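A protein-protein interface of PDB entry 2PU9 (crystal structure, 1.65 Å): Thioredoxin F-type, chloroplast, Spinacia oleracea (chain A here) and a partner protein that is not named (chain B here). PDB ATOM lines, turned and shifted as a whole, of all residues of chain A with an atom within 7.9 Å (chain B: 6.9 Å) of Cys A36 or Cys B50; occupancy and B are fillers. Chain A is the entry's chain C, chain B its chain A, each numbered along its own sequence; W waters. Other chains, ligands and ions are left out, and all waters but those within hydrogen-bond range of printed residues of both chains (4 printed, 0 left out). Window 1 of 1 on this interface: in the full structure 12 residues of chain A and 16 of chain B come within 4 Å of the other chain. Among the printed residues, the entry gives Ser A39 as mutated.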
ATOM      1  N   MET A  31     -16.286  -5.180  -1.106  1.00  0.00           N
ATOM      2  CA  MET A  31     -17.231  -6.139  -0.538  1.00  0.00           C
ATOM      3  C   MET A  31     -16.851  -6.298   0.923  1.00  0.00           C
ATOM      4  O   MET A  31     -15.790  -6.817   1.241  1.00  0.00           O
ATOM      5  CB  MET A  31     -17.135  -7.468  -1.288  1.00  0.00           C
ATOM      6  CG  MET A  31     -17.536  -7.336  -2.745  1.00  0.00           C
ATOM      7  SD  MET A  31     -17.365  -8.886  -3.665  1.00  0.00           S
ATOM      8  CE  MET A  31     -18.845  -9.734  -3.183  1.00  0.00           C
ATOM      9  N   PHE A  32     -17.721  -5.831   1.811  1.00  0.00           N
ATOM     10  CA  PHE A  32     -17.437  -5.868   3.242  1.00  0.00           C
ATOM     11  C   PHE A  32     -18.622  -6.340   4.067  1.00  0.00           C
ATOM     12  O   PHE A  32     -19.690  -6.628   3.541  1.00  0.00           O
ATOM     13  CB  PHE A  32     -17.100  -4.456   3.724  1.00  0.00           C
ATOM     14  CG  PHE A  32     -18.293  -3.527   3.735  1.00  0.00           C
ATOM     15  CD1 PHE A  32     -18.789  -2.991   2.549  1.00  0.00           C
ATOM     16  CD2 PHE A  32     -18.963  -3.245   4.926  1.00  0.00           C
ATOM     17  CE1 PHE A  32     -19.934  -2.192   2.544  1.00  0.00           C
ATOM     18  CE2 PHE A  32     -20.109  -2.445   4.932  1.00  0.00           C
ATOM     19  CZ  PHE A  32     -20.598  -1.919   3.740  1.00  0.00           C
ATOM     20  N   THR A  33     -18.397  -6.404   5.378  1.00  0.00           N
ATOM     21  CA  THR A  33     -19.426  -6.736   6.359  1.00  0.00           C
ATOM     22  C   THR A  33     -19.168  -5.717   7.464  1.00  0.00           C
ATOM     23  O   THR A  33     -18.031  -5.288   7.661  1.00  0.00           O
ATOM     24  CB  THR A  33     -19.299  -8.168   6.927  1.00  0.00           C
ATOM     25  OG1 THR A  33     -18.033  -8.328   7.574  1.00  0.00           O
ATOM     26  CG2 THR A  33     -19.446  -9.188   5.814  1.00  0.00           C
ATOM     27  N   GLN A  34     -20.218  -5.320   8.170  1.00  0.00           N
ATOM     28  CA  GLN A  34     -20.086  -4.323   9.225  1.00  0.00           C
ATOM     29  C   GLN A  34     -19.185  -4.712  10.386  1.00  0.00           C
ATOM     30  O   GLN A  34     -18.447  -3.880  10.916  1.00  0.00           O
ATOM     31  CB  GLN A  34     -21.463  -3.962   9.785  1.00  0.00           C
ATOM     32  CG  GLN A  34     -22.351  -3.178   8.842  1.00  0.00           C
ATOM     33  CD  GLN A  34     -23.645  -2.752   9.503  1.00  0.00           C
ATOM     34  OE1 GLN A  34     -23.634  -2.079  10.536  1.00  0.00           O
ATOM     35  NE2 GLN A  34     -24.769  -3.141   8.912  1.00  0.00           N
ATOM     36  N   TRP A  35     -19.240  -5.975  10.787  1.00  0.00           N
ATOM     37  CA  TRP A  35     -18.460  -6.415  11.935  1.00  0.00           C
ATOM     38  C   TRP A  35     -17.167  -7.140  11.586  1.00  0.00           C
ATOM     39  O   TRP A  35     -16.882  -8.220  12.101  1.00  0.00           O
ATOM     40  CB  TRP A  35     -19.368  -7.265  12.831  1.00  0.00           C
ATOM     41  CG  TRP A  35     -20.689  -6.579  13.047  1.00  0.00           C
ATOM     42  CD1 TRP A  35     -21.882  -6.870  12.439  1.00  0.00           C
ATOM     43  CD2 TRP A  35     -20.922  -5.410  13.841  1.00  0.00           C
ATOM     44  NE1 TRP A  35     -22.839  -5.947  12.803  1.00  0.00           N
ATOM     45  CE2 TRP A  35     -22.276  -5.040  13.661  1.00  0.00           C
ATOM     46  CE3 TRP A  35     -20.116  -4.635  14.684  1.00  0.00           C
ATOM     47  CZ2 TRP A  35     -22.839  -3.928  14.297  1.00  0.00           C
ATOM     48  CZ3 TRP A  35     -20.676  -3.529  15.315  1.00  0.00           C
ATOM     49  CH2 TRP A  35     -22.026  -3.187  15.117  1.00  0.00           C
ATOM     50  N   CYS A  36     -16.383  -6.511  10.714  1.00  0.00           N
ATOM     51  CA  CYS A  36     -15.105  -7.048  10.262  1.00  0.00           C
ATOM     52  C   CYS A  36     -13.988  -6.038  10.527  1.00  0.00           C
ATOM     53  O   CYS A  36     -14.042  -4.906  10.047  1.00  0.00           O
ATOM     54  CB  CYS A  36     -15.177  -7.366   8.767  1.00  0.00           C
ATOM     55  SG  CYS A  36     -13.587  -7.790   8.033  1.00  0.00           S
ATOM     56  N   GLY A  37     -12.977  -6.468  11.279  1.00  0.00           N
ATOM     57  CA  GLY A  37     -11.858  -5.609  11.631  1.00  0.00           C
ATOM     58  C   GLY A  37     -11.074  -5.003  10.482  1.00  0.00           C
ATOM     59  O   GLY A  37     -11.009  -3.778  10.362  1.00  0.00           O
ATOM     60  N   PRO A  38     -10.452  -5.825   9.626  1.00  0.00           N
ATOM     61  CA  PRO A  38      -9.688  -5.263   8.508  1.00  0.00           C
ATOM     62  C   PRO A  38     -10.529  -4.357   7.611  1.00  0.00           C
ATOM     63  O   PRO A  38     -10.021  -3.387   7.053  1.00  0.00           O
ATOM     64  CB  PRO A  38      -9.156  -6.506   7.786  1.00  0.00           C
ATOM     65  CG  PRO A  38     -10.142  -7.588   8.154  1.00  0.00           C
ATOM     66  CD  PRO A  38     -10.418  -7.297   9.608  1.00  0.00           C
ATOM     67  N   SER A  39     -11.814  -4.664   7.487  1.00  0.00           N
ATOM     68  CA  SER A  39     -12.701  -3.858   6.661  1.00  0.00           C
ATOM     69  C   SER A  39     -12.861  -2.459   7.262  1.00  0.00           C
ATOM     70  O   SER A  39     -12.815  -1.457   6.549  1.00  0.00           O
ATOM     71  CB  SER A  39     -14.066  -4.537   6.545  1.00  0.00           C
ATOM     72  OG  SER A  39     -14.948  -3.766   5.752  1.00  0.00           O
ATOM     73  N   LYS A  40     -13.037  -2.397   8.579  1.00  0.00           N
ATOM     74  CA  LYS A  40     -13.196  -1.117   9.260  1.00  0.00           C
ATOM     75  C   LYS A  40     -11.903  -0.312   9.189  1.00  0.00           C
ATOM     76  O   LYS A  40     -11.928   0.905   9.014  1.00  0.00           O
ATOM     77  CB  LYS A  40     -13.584  -1.334  10.725  1.00  0.00           C
ATOM     78  CG  LYS A  40     -14.060  -0.066  11.421  1.00  0.00           C
ATOM     79  CD  LYS A  40     -14.523  -0.351  12.841  1.00  0.00           C
ATOM     80  CE  LYS A  40     -15.202   0.866  13.447  1.00  0.00           C
ATOM     81  NZ  LYS A  40     -14.308   2.056  13.450  1.00  0.00           N
ATOM     82  N   ALA A  41     -10.773  -0.996   9.320  1.00  0.00           N
ATOM     83  CA  ALA A  41      -9.476  -0.331   9.272  1.00  0.00           C
ATOM     84  C   ALA A  41      -9.240   0.315   7.909  1.00  0.00           C
ATOM     85  O   ALA A  41      -8.681   1.408   7.817  1.00  0.00           O
ATOM     86  CB  ALA A  41      -8.364  -1.332   9.578  1.00  0.00           C
ATOM     87  N   MET A  42      -9.683  -0.370   6.860  1.00  0.00           N
ATOM     88  CA  MET A  42      -9.527   0.090   5.480  1.00  0.00           C
ATOM     89  C   MET A  42     -10.446   1.237   5.065  1.00  0.00           C
ATOM     90  O   MET A  42     -10.101   2.019   4.180  1.00  0.00           O
ATOM     91  CB  MET A  42      -9.766  -1.074   4.518  1.00  0.00           C
ATOM     92  CG  MET A  42      -8.649  -2.086   4.447  1.00  0.00           C
ATOM     93  SD  MET A  42      -7.288  -1.503   3.431  1.00  0.00           S
ATOM     94  CE  MET A  42      -7.965  -1.745   1.811  1.00  0.00           C
ATOM     95  N   ILE A  76     -16.939 -14.164  -2.915  1.00  0.00           N
ATOM     96  CA  ILE A  76     -16.159 -13.573  -1.831  1.00  0.00           C
ATOM     97  C   ILE A  76     -15.963 -14.614  -0.737  1.00  0.00           C
ATOM     98  O   ILE A  76     -16.905 -15.309  -0.354  1.00  0.00           O
ATOM     99  CB  ILE A  76     -16.858 -12.328  -1.223  1.00  0.00           C
ATOM    100  CG1 ILE A  76     -16.073 -11.840   0.001  1.00  0.00           C
ATOM    101  CG2 ILE A  76     -18.297 -12.664  -0.855  1.00  0.00           C
ATOM    102  CD1 ILE A  76     -16.591 -10.541   0.611  1.00  0.00           C
ATOM    103  N   ARG A  77     -14.730 -14.733  -0.257  1.00  0.00           N
ATOM    104  CA  ARG A  77     -14.401 -15.671   0.806  1.00  0.00           C
ATOM    105  C   ARG A  77     -13.795 -14.859   1.940  1.00  0.00           C
ATOM    106  O   ARG A  77     -14.206 -14.971   3.094  1.00  0.00           O
ATOM    107  CB  ARG A  77     -13.376 -16.706   0.334  1.00  0.00           C
ATOM    108  CG  ARG A  77     -13.832 -17.592  -0.803  1.00  0.00           C
ATOM    109  CD  ARG A  77     -12.761 -18.627  -1.120  1.00  0.00           C
ATOM    110  NE  ARG A  77     -11.453 -18.010  -1.333  1.00  0.00           N
ATOM    111  CZ  ARG A  77     -11.147 -17.231  -2.367  1.00  0.00           C
ATOM    112  NH1 ARG A  77     -12.055 -16.970  -3.297  1.00  0.00           N
ATOM    113  NH2 ARG A  77      -9.932 -16.705  -2.467  1.00  0.00           N
ATOM    114  N   VAL A  78     -12.805 -14.044   1.592  1.00  0.00           N
ATOM    115  CA  VAL A  78     -12.128 -13.195   2.563  1.00  0.00           C
ATOM    116  C   VAL A  78     -12.829 -11.849   2.646  1.00  0.00           C
ATOM    117  O   VAL A  78     -13.188 -11.274   1.621  1.00  0.00           O
ATOM    118  CB  VAL A  78     -10.669 -12.923   2.143  1.00  0.00           C
ATOM    119  CG1 VAL A  78      -9.961 -12.092   3.210  1.00  0.00           C
ATOM    120  CG2 VAL A  78      -9.942 -14.233   1.911  1.00  0.00           C
ATOM    121  N   VAL A  79     -13.035 -11.351   3.862  1.00  0.00           N
ATOM    122  CA  VAL A  79     -13.650 -10.041   4.032  1.00  0.00           C
ATOM    123  C   VAL A  79     -12.554  -9.111   4.552  1.00  0.00           C
ATOM    124  O   VAL A  79     -11.872  -9.435   5.521  1.00  0.00           O
ATOM    125  CB  VAL A  79     -14.822 -10.063   5.048  1.00  0.00           C
ATOM    126  CG1 VAL A  79     -15.494  -8.684   5.090  1.00  0.00           C
ATOM    127  CG2 VAL A  79     -15.842 -11.123   4.651  1.00  0.00           C
ATOM    128  N   PRO A  80     -12.334  -7.968   3.884  1.00  0.00           N
ATOM    129  CA  PRO A  80     -13.042  -7.514   2.689  1.00  0.00           C
ATOM    130  C   PRO A  80     -12.363  -8.059   1.436  1.00  0.00           C
ATOM    131  O   PRO A  80     -11.255  -8.601   1.499  1.00  0.00           O
ATOM    132  CB  PRO A  80     -12.904  -6.001   2.778  1.00  0.00           C
ATOM    133  CG  PRO A  80     -11.486  -5.863   3.257  1.00  0.00           C
ATOM    134  CD  PRO A  80     -11.382  -6.937   4.344  1.00  0.00           C
ATOM    135  N   THR A  81     -13.045  -7.916   0.308  1.00  0.00           N
ATOM    136  CA  THR A  81     -12.513  -8.320  -0.983  1.00  0.00           C
ATOM    137  C   THR A  81     -12.898  -7.208  -1.941  1.00  0.00           C
ATOM    138  O   THR A  81     -14.036  -6.750  -1.941  1.00  0.00           O
ATOM    139  CB  THR A  81     -13.102  -9.655  -1.470  1.00  0.00           C
ATOM    140  OG1 THR A  81     -12.452 -10.730  -0.783  1.00  0.00           O
ATOM    141  CG2 THR A  81     -12.893  -9.826  -2.978  1.00  0.00           C
ATOM    142  N   GLY A  96      -8.630  -9.192   1.086  1.00  0.00           N
ATOM    143  CA  GLY A  96      -8.046  -8.729   2.331  1.00  0.00           C
ATOM    144  C   GLY A  96      -7.803  -7.233   2.340  1.00  0.00           C
ATOM    145  O   GLY A  96      -7.987  -6.558   1.324  1.00  0.00           O
ATOM    146  N   ALA A  97      -7.390  -6.714   3.490  1.00  0.00           N
ATOM    147  CA  ALA A  97      -7.120  -5.289   3.642  1.00  0.00           C
ATOM    148  C   ALA A  97      -5.708  -4.966   3.164  1.00  0.00           C
ATOM    149  O   ALA A  97      -4.856  -4.562   3.955  1.00  0.00           O
ATOM    150  CB  ALA A  97      -7.280  -4.889   5.099  1.00  0.00           C
ATOM    151  N   VAL B  28     -11.486  -1.578  16.107  1.00  0.00           N
ATOM    152  CA  VAL B  28     -11.293  -2.783  15.300  1.00  0.00           C
ATOM    153  C   VAL B  28     -11.621  -3.985  16.185  1.00  0.00           C
ATOM    154  O   VAL B  28     -12.367  -4.881  15.805  1.00  0.00           O
ATOM    155  CB  VAL B  28      -9.823  -2.872  14.803  1.00  0.00           C
ATOM    156  CG1 VAL B  28      -9.537  -4.238  14.203  1.00  0.00           C
ATOM    157  CG2 VAL B  28      -9.572  -1.789  13.770  1.00  0.00           C
ATOM    158  N   VAL B  31     -15.592  -4.287  16.883  1.00  0.00           N
ATOM    159  CA  VAL B  31     -16.476  -4.812  15.849  1.00  0.00           C
ATOM    160  C   VAL B  31     -16.318  -6.313  15.654  1.00  0.00           C
ATOM    161  O   VAL B  31     -17.294  -7.007  15.376  1.00  0.00           O
ATOM    162  CB  VAL B  31     -16.292  -4.083  14.488  1.00  0.00           C
ATOM    163  CG1 VAL B  31     -16.577  -2.599  14.662  1.00  0.00           C
ATOM    164  CG2 VAL B  31     -14.893  -4.302  13.942  1.00  0.00           C
ATOM    165  N   VAL B  32     -15.100  -6.819  15.822  1.00  0.00           N
ATOM    166  CA  VAL B  32     -14.875  -8.247  15.661  1.00  0.00           C
ATOM    167  C   VAL B  32     -15.564  -9.024  16.771  1.00  0.00           C
ATOM    168  O   VAL B  32     -16.150 -10.076  16.527  1.00  0.00           O
ATOM    169  CB  VAL B  32     -13.378  -8.590  15.669  1.00  0.00           C
ATOM    170  CG1 VAL B  32     -13.202 -10.104  15.635  1.00  0.00           C
ATOM    171  CG2 VAL B  32     -12.698  -7.953  14.470  1.00  0.00           C
ATOM    172  N   GLY B  35     -19.180  -9.140  16.009  1.00  0.00           N
ATOM    173  CA  GLY B  35     -19.408 -10.059  14.908  1.00  0.00           C
ATOM    174  C   GLY B  35     -19.382 -11.502  15.374  1.00  0.00           C
ATOM    175  O   GLY B  35     -20.195 -12.326  14.940  1.00  0.00           O
ATOM    176  N   HIS B  39     -22.649 -14.254  15.449  1.00  0.00           N
ATOM    177  CA  HIS B  39     -22.622 -15.597  14.889  1.00  0.00           C
ATOM    178  C   HIS B  39     -22.920 -16.647  15.946  1.00  0.00           C
ATOM    179  O   HIS B  39     -23.635 -17.613  15.681  1.00  0.00           O
ATOM    180  CB  HIS B  39     -21.267 -15.869  14.232  1.00  0.00           C
ATOM    181  CG  HIS B  39     -21.165 -15.333  12.839  1.00  0.00           C
ATOM    182  ND1 HIS B  39     -19.965 -15.202  12.176  1.00  0.00           N
ATOM    183  CD2 HIS B  39     -22.121 -14.912  11.976  1.00  0.00           C
ATOM    184  CE1 HIS B  39     -20.185 -14.724  10.964  1.00  0.00           C
ATOM    185  NE2 HIS B  39     -21.485 -14.539  10.817  1.00  0.00           N
ATOM    186  N   LEU B  47     -18.488 -18.330  14.418  1.00  0.00           N
ATOM    187  CA  LEU B  47     -17.789 -18.356  13.139  1.00  0.00           C
ATOM    188  C   LEU B  47     -17.107 -17.010  12.932  1.00  0.00           C
ATOM    189  O   LEU B  47     -17.650 -15.963  13.296  1.00  0.00           O
ATOM    190  CB  LEU B  47     -18.763 -18.590  11.979  1.00  0.00           C
ATOM    191  CG  LEU B  47     -19.254 -20.003  11.674  1.00  0.00           C
ATOM    192  CD1 LEU B  47     -20.171 -19.949  10.462  1.00  0.00           C
ATOM    193  CD2 LEU B  47     -18.066 -20.919  11.393  1.00  0.00           C
ATOM    194  N   CYS B  48     -15.915 -17.040  12.354  1.00  0.00           N
ATOM    195  CA  CYS B  48     -15.175 -15.817  12.092  1.00  0.00           C
ATOM    196  C   CYS B  48     -16.039 -14.805  11.342  1.00  0.00           C
ATOM    197  O   CYS B  48     -16.685 -15.148  10.347  1.00  0.00           O
ATOM    198  CB  CYS B  48     -13.932 -16.141  11.270  1.00  0.00           C
ATOM    199  SG  CYS B  48     -12.906 -14.708  10.990  1.00  0.00           S
ATOM    200  N   PRO B  49     -16.061 -13.542  11.804  1.00  0.00           N
ATOM    201  CA  PRO B  49     -16.869 -12.524  11.130  1.00  0.00           C
ATOM    202  C   PRO B  49     -16.192 -11.853   9.936  1.00  0.00           C
ATOM    203  O   PRO B  49     -16.790 -10.992   9.291  1.00  0.00           O
ATOM    204  CB  PRO B  49     -17.170 -11.535  12.255  1.00  0.00           C
ATOM    205  CG  PRO B  49     -15.885 -11.540  13.022  1.00  0.00           C
ATOM    206  CD  PRO B  49     -15.545 -13.030  13.090  1.00  0.00           C
ATOM    207  N   CYS B  50     -14.956 -12.248   9.642  1.00  0.00           N
ATOM    208  CA  CYS B  50     -14.218 -11.666   8.524  1.00  0.00           C
ATOM    209  C   CYS B  50     -14.031 -12.641   7.374  1.00  0.00           C
ATOM    210  O   CYS B  50     -13.080 -12.530   6.596  1.00  0.00           O
ATOM    211  CB  CYS B  50     -12.861 -11.142   8.990  1.00  0.00           C
ATOM    212  SG  CYS B  50     -12.997  -9.824  10.225  1.00  0.00           S
ATOM    213  N   ARG B  51     -14.943 -13.602   7.294  1.00  0.00           N
ATOM    214  CA  ARG B  51     -14.968 -14.597   6.227  1.00  0.00           C
ATOM    215  C   ARG B  51     -16.410 -14.618   5.749  1.00  0.00           C
ATOM    216  O   ARG B  51     -17.329 -14.366   6.533  1.00  0.00           O
ATOM    217  CB  ARG B  51     -14.633 -16.003   6.742  1.00  0.00           C
ATOM    218  CG  ARG B  51     -13.225 -16.199   7.285  1.00  0.00           C
ATOM    219  CD  ARG B  51     -12.144 -16.047   6.220  1.00  0.00           C
ATOM    220  NE  ARG B  51     -12.331 -16.940   5.081  1.00  0.00           N
ATOM    221  CZ  ARG B  51     -11.383 -17.206   4.186  1.00  0.00           C
ATOM    222  NH1 ARG B  51     -10.181 -16.651   4.305  1.00  0.00           N
ATOM    223  NH2 ARG B  51     -11.639 -18.018   3.169  1.00  0.00           N
ATOM    224  N   HIS B  52     -16.610 -14.890   4.464  1.00  0.00           N
ATOM    225  CA  HIS B  52     -17.958 -15.005   3.929  1.00  0.00           C
ATOM    226  C   HIS B  52     -18.150 -16.488   3.676  1.00  0.00           C
ATOM    227  O   HIS B  52     -17.231 -17.162   3.208  1.00  0.00           O
ATOM    228  CB  HIS B  52     -18.126 -14.258   2.607  1.00  0.00           C
ATOM    229  CG  HIS B  52     -19.468 -14.467   1.979  1.00  0.00           C
ATOM    230  ND1 HIS B  52     -20.610 -13.848   2.445  1.00  0.00           N
ATOM    231  CD2 HIS B  52     -19.867 -15.282   0.974  1.00  0.00           C
ATOM    232  CE1 HIS B  52     -21.652 -14.276   1.755  1.00  0.00           C
ATOM    233  NE2 HIS B  52     -21.229 -15.148   0.858  1.00  0.00           N
ATOM    234  N   TYR B  53     -19.336 -16.996   3.980  1.00  0.00           N
ATOM    235  CA  TYR B  53     -19.604 -18.416   3.796  1.00  0.00           C
ATOM    236  C   TYR B  53     -20.768 -18.684   2.856  1.00  0.00           C
ATOM    237  O   TYR B  53     -21.734 -17.931   2.832  1.00  0.00           O
ATOM    238  CB  TYR B  53     -19.901 -19.058   5.148  1.00  0.00           C
ATOM    239  CG  TYR B  53     -18.938 -18.640   6.239  1.00  0.00           C
ATOM    240  CD1 TYR B  53     -19.269 -17.627   7.143  1.00  0.00           C
ATOM    241  CD2 TYR B  53     -17.689 -19.247   6.359  1.00  0.00           C
ATOM    242  CE1 TYR B  53     -18.370 -17.231   8.143  1.00  0.00           C
ATOM    243  CE2 TYR B  53     -16.788 -18.860   7.351  1.00  0.00           C
ATOM    244  CZ  TYR B  53     -17.134 -17.854   8.237  1.00  0.00           C
ATOM    245  OH  TYR B  53     -16.240 -17.476   9.216  1.00  0.00           O
ATOM    246  N   HIS B  79      -6.788 -13.093  10.979  1.00  0.00           N
ATOM    247  CA  HIS B  79      -7.128 -12.174   9.901  1.00  0.00           C
ATOM    248  C   HIS B  79      -8.032 -11.025  10.353  1.00  0.00           C
ATOM    249  O   HIS B  79      -7.969  -9.927   9.803  1.00  0.00           O
ATOM    250  CB  HIS B  79      -7.809 -12.947   8.767  1.00  0.00           C
ATOM    251  CG  HIS B  79      -8.446 -12.069   7.734  1.00  0.00           C
ATOM    252  ND1 HIS B  79      -7.722 -11.201   6.945  1.00  0.00           N
ATOM    253  CD2 HIS B  79      -9.743 -11.911   7.377  1.00  0.00           C
ATOM    254  CE1 HIS B  79      -8.547 -10.542   6.148  1.00  0.00           C
ATOM    255  NE2 HIS B  79      -9.778 -10.954   6.391  1.00  0.00           N
ATOM    256  N   CYS B  80      -8.864 -11.279  11.357  1.00  0.00           N
ATOM    257  CA  CYS B  80      -9.786 -10.263  11.868  1.00  0.00           C
ATOM    258  C   CYS B  80      -9.088  -9.135  12.600  1.00  0.00           C
ATOM    259  O   CYS B  80      -9.706  -8.114  12.884  1.00  0.00           O
ATOM    260  CB  CYS B  80     -10.799 -10.883  12.838  1.00  0.00           C
ATOM    261  SG  CYS B  80     -12.008 -11.954  12.063  1.00  0.00           S
ATOM    262  N   MET B  81      -7.807  -9.328  12.902  1.00  0.00           N
ATOM    263  CA  MET B  81      -7.026  -8.341  13.636  1.00  0.00           C
ATOM    264  C   MET B  81      -7.515  -8.223  15.075  1.00  0.00           C
ATOM    265  O   MET B  81      -7.422  -7.157  15.688  1.00  0.00           O
ATOM    266  CB  MET B  81      -7.083  -6.980  12.942  1.00  0.00           C
ATOM    267  CG  MET B  81      -6.312  -6.937  11.633  1.00  0.00           C
ATOM    268  SD  MET B  81      -6.576  -5.407  10.709  1.00  0.00           S
ATOM    269  CE  MET B  81      -5.680  -4.226  11.717  1.00  0.00           C
ATOM    270  N   MET B 109     -22.139   2.550  14.766  1.00  0.00           N
ATOM    271  CA  MET B 109     -22.498   1.873  13.527  1.00  0.00           C
ATOM    272  C   MET B 109     -23.954   2.132  13.150  1.00  0.00           C
ATOM    273  O   MET B 109     -24.379   1.830  12.032  1.00  0.00           O
ATOM    274  CB  MET B 109     -22.268   0.366  13.673  1.00  0.00           C
ATOM    275  CG  MET B 109     -20.863  -0.010  14.109  1.00  0.00           C
ATOM    276  SD  MET B 109     -19.621   0.295  12.843  1.00  0.00           S
ATOM    277  CE  MET B 109     -19.638  -1.282  11.989  1.00  0.00           C
HETATM  278  O   HOH W   1      -6.344  -8.491   5.544  1.00  0.00           O
HETATM  279  O   HOH W   2     -22.724   0.880   9.673  1.00  0.00           O
HETATM  280  O   HOH W   3     -25.607  -1.285  12.945  1.00  0.00           O
HETATM  281  O   HOH W   4     -14.663 -18.209   3.858  1.00  0.00           O
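The backbone NH (N) of Gly A37 sits at hydrogen-bond distance from the side-chain sulfur (SG) of Cys B50 (3.5 Å).
The guanidinium group of Arg B51 sits close to the backbone carbonyl oxygen of Arg A77.
The backbone carbonyl oxygen (O) of Val A79 lies within hydrogen-bond range of a ring nitrogen (NE2) of His B79, at 2.7 Å.
O of Cys B50 lies within hydrogen-bond range of N of Val A79, at 3.0 Å.
SG of Cys A36 lies close to SG of Cys B50.
The backbone carbonyl oxygen (O) of Pro B49 is in hydrogen-bond range of the side-chain hydroxyl (OG1) of Thr A33 (3.4 Å).
The backbone carbonyl oxygen (O) of Arg A77 is in hydrogen-bond range of the backbone NH (N) of His B52.
SG of Cys B48 lies close to SG of Cys B80 (3.1 Å).
The backbone carbonyl oxygen (O) of Val A78 sits at hydrogen-bond distance from the side-chain hydroxyl (OG1) of Thr A81 (2.6 Å).
SG of Cys A36 lies close to N of Ser A39 (3.6 Å).
The side-chain sulfur (SG) of Cys A36 lies within hydrogen-bond range of the backbone carbonyl oxygen (O) of Val A79, at 3.5 Å.
N of Cys B50 lies close to SG of Cys B48, at 3.5 Å.
Of the 20 printed residues of chain A, 11 touch a printed residue of chain B.
Printed residues of chain A that touch a printed residue of chain B: Thr A33, Gln A34, Trp A35, Cys A36, Gly A37, Pro A38, Lys A40, Ile A76, Arg A77, Val A78 and Val A79.
Hydrophobic or aromatic side chains of chain A within 4 Å of the printed part of chain B: Trp A35, Pro A38, Ile A76, Val A78 and Val A79.
Of the 16 printed residues of chain B, 12 touch a printed residue of chain A.
Printed residues of chain B that touch a printed residue of chain A: Val B28, Val B31, Val B32, Gly B35, Pro B49, Cys B50, Arg B51, His B52, His B79, Cys B80, Met B81 and Met B109.
Hydrophobic or aromatic side chains of chain B within 4 Å of the printed part of chain A: Val B28, Val B31, Val B32, Pro B49, His B52, His B79, Met B81 and Met B109.
Among the printed residues, no Asp or Glu carboxylate lies within 4 Å of a Lys or Arg side-chain nitrogen of the other chain.
Among the printed residues, merely in contact across the chains: Gln A34 with Met B109 (3.1 Å), Trp A35 with Val B31 (3.3 Å), Trp A35 with Gly B35 (3.5 Å), Trp A35 with Pro B49 (3.3 Å), Trp A35 with Met B109 (3.5 Å), Cys A36 with Val B31 (3.9 Å), Gly A37 with Val B28 (3.7 Å), Gly A37 with Val B31 (3.9 Å), Gly A37 with Val B32 (3.5 Å), Gly A37 with Cys B80 (3.5 Å), Pro A38 with Cys B50 (3.7 Å), Pro A38 with His B79 (3.6 Å), Pro A38 with Cys B80 (3.5 Å), Pro A38 with Met B81 (3.8 Å), Lys A40 with Val B31 (3.5 Å), Ile A76 with His B52 (3.2 Å), Val A78 with Arg B51 (3.4 Å), Val A78 with His B79 (3.4 Å), Val A79 with Arg B51 (3.7 Å) and Val A79 with His B52 (3.8 Å).
Of the printed residues of chain B, Gln A34 touches Met B109.
Printed residues of chain B within 4 Å of Cys A36: Val B31 and Cys B50.
Of the printed residues of chain A, Val B32 touches Gly A37 (3.5 Å).
Printed residues of chain A within 4 Å of Cys B50: Cys A36 (3.0 Å), Gly A37 (3.5 Å), Pro A38 (3.7 Å) and Val A79 (3.0 Å).
Printed residues of chain A within 4 Å of Arg B51: Arg A77, Val A78 and Val A79.
Of the printed residues of chain A, His B79 touches Pro A38, Val A78 and Val A79.
Printed residues of chain A within 4 Å of Cys B80: Gly A37 (3.5 Å) and Pro A38 (3.5 Å).
The nearest printed residue of chain A that does not touch Val B31 is Gln A34 (4.2 Å).
Water W4 lies within hydrogen-bond range of the backbone carbonyl oxygen (O) of His B52 (2.8 Å), the guanidinium group (NE) of Arg B51 (2.9 Å) and the backbone carbonyl oxygen (O) of Arg A77 (3.4 Å).
Water W1 lies within hydrogen-bond range of the backbone NH (N) of Ala A97 (2.9 Å) and a ring nitrogen (ND1) of His B79 (3.3 Å).
Water W2 bridges O of Met B109 (3.0 Å) and OE1 of Gln A34 (3.2 Å).
Water W3 bridges OE1 of Gln A34 (3.2 Å) and O of Met B109 (3.5 Å).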
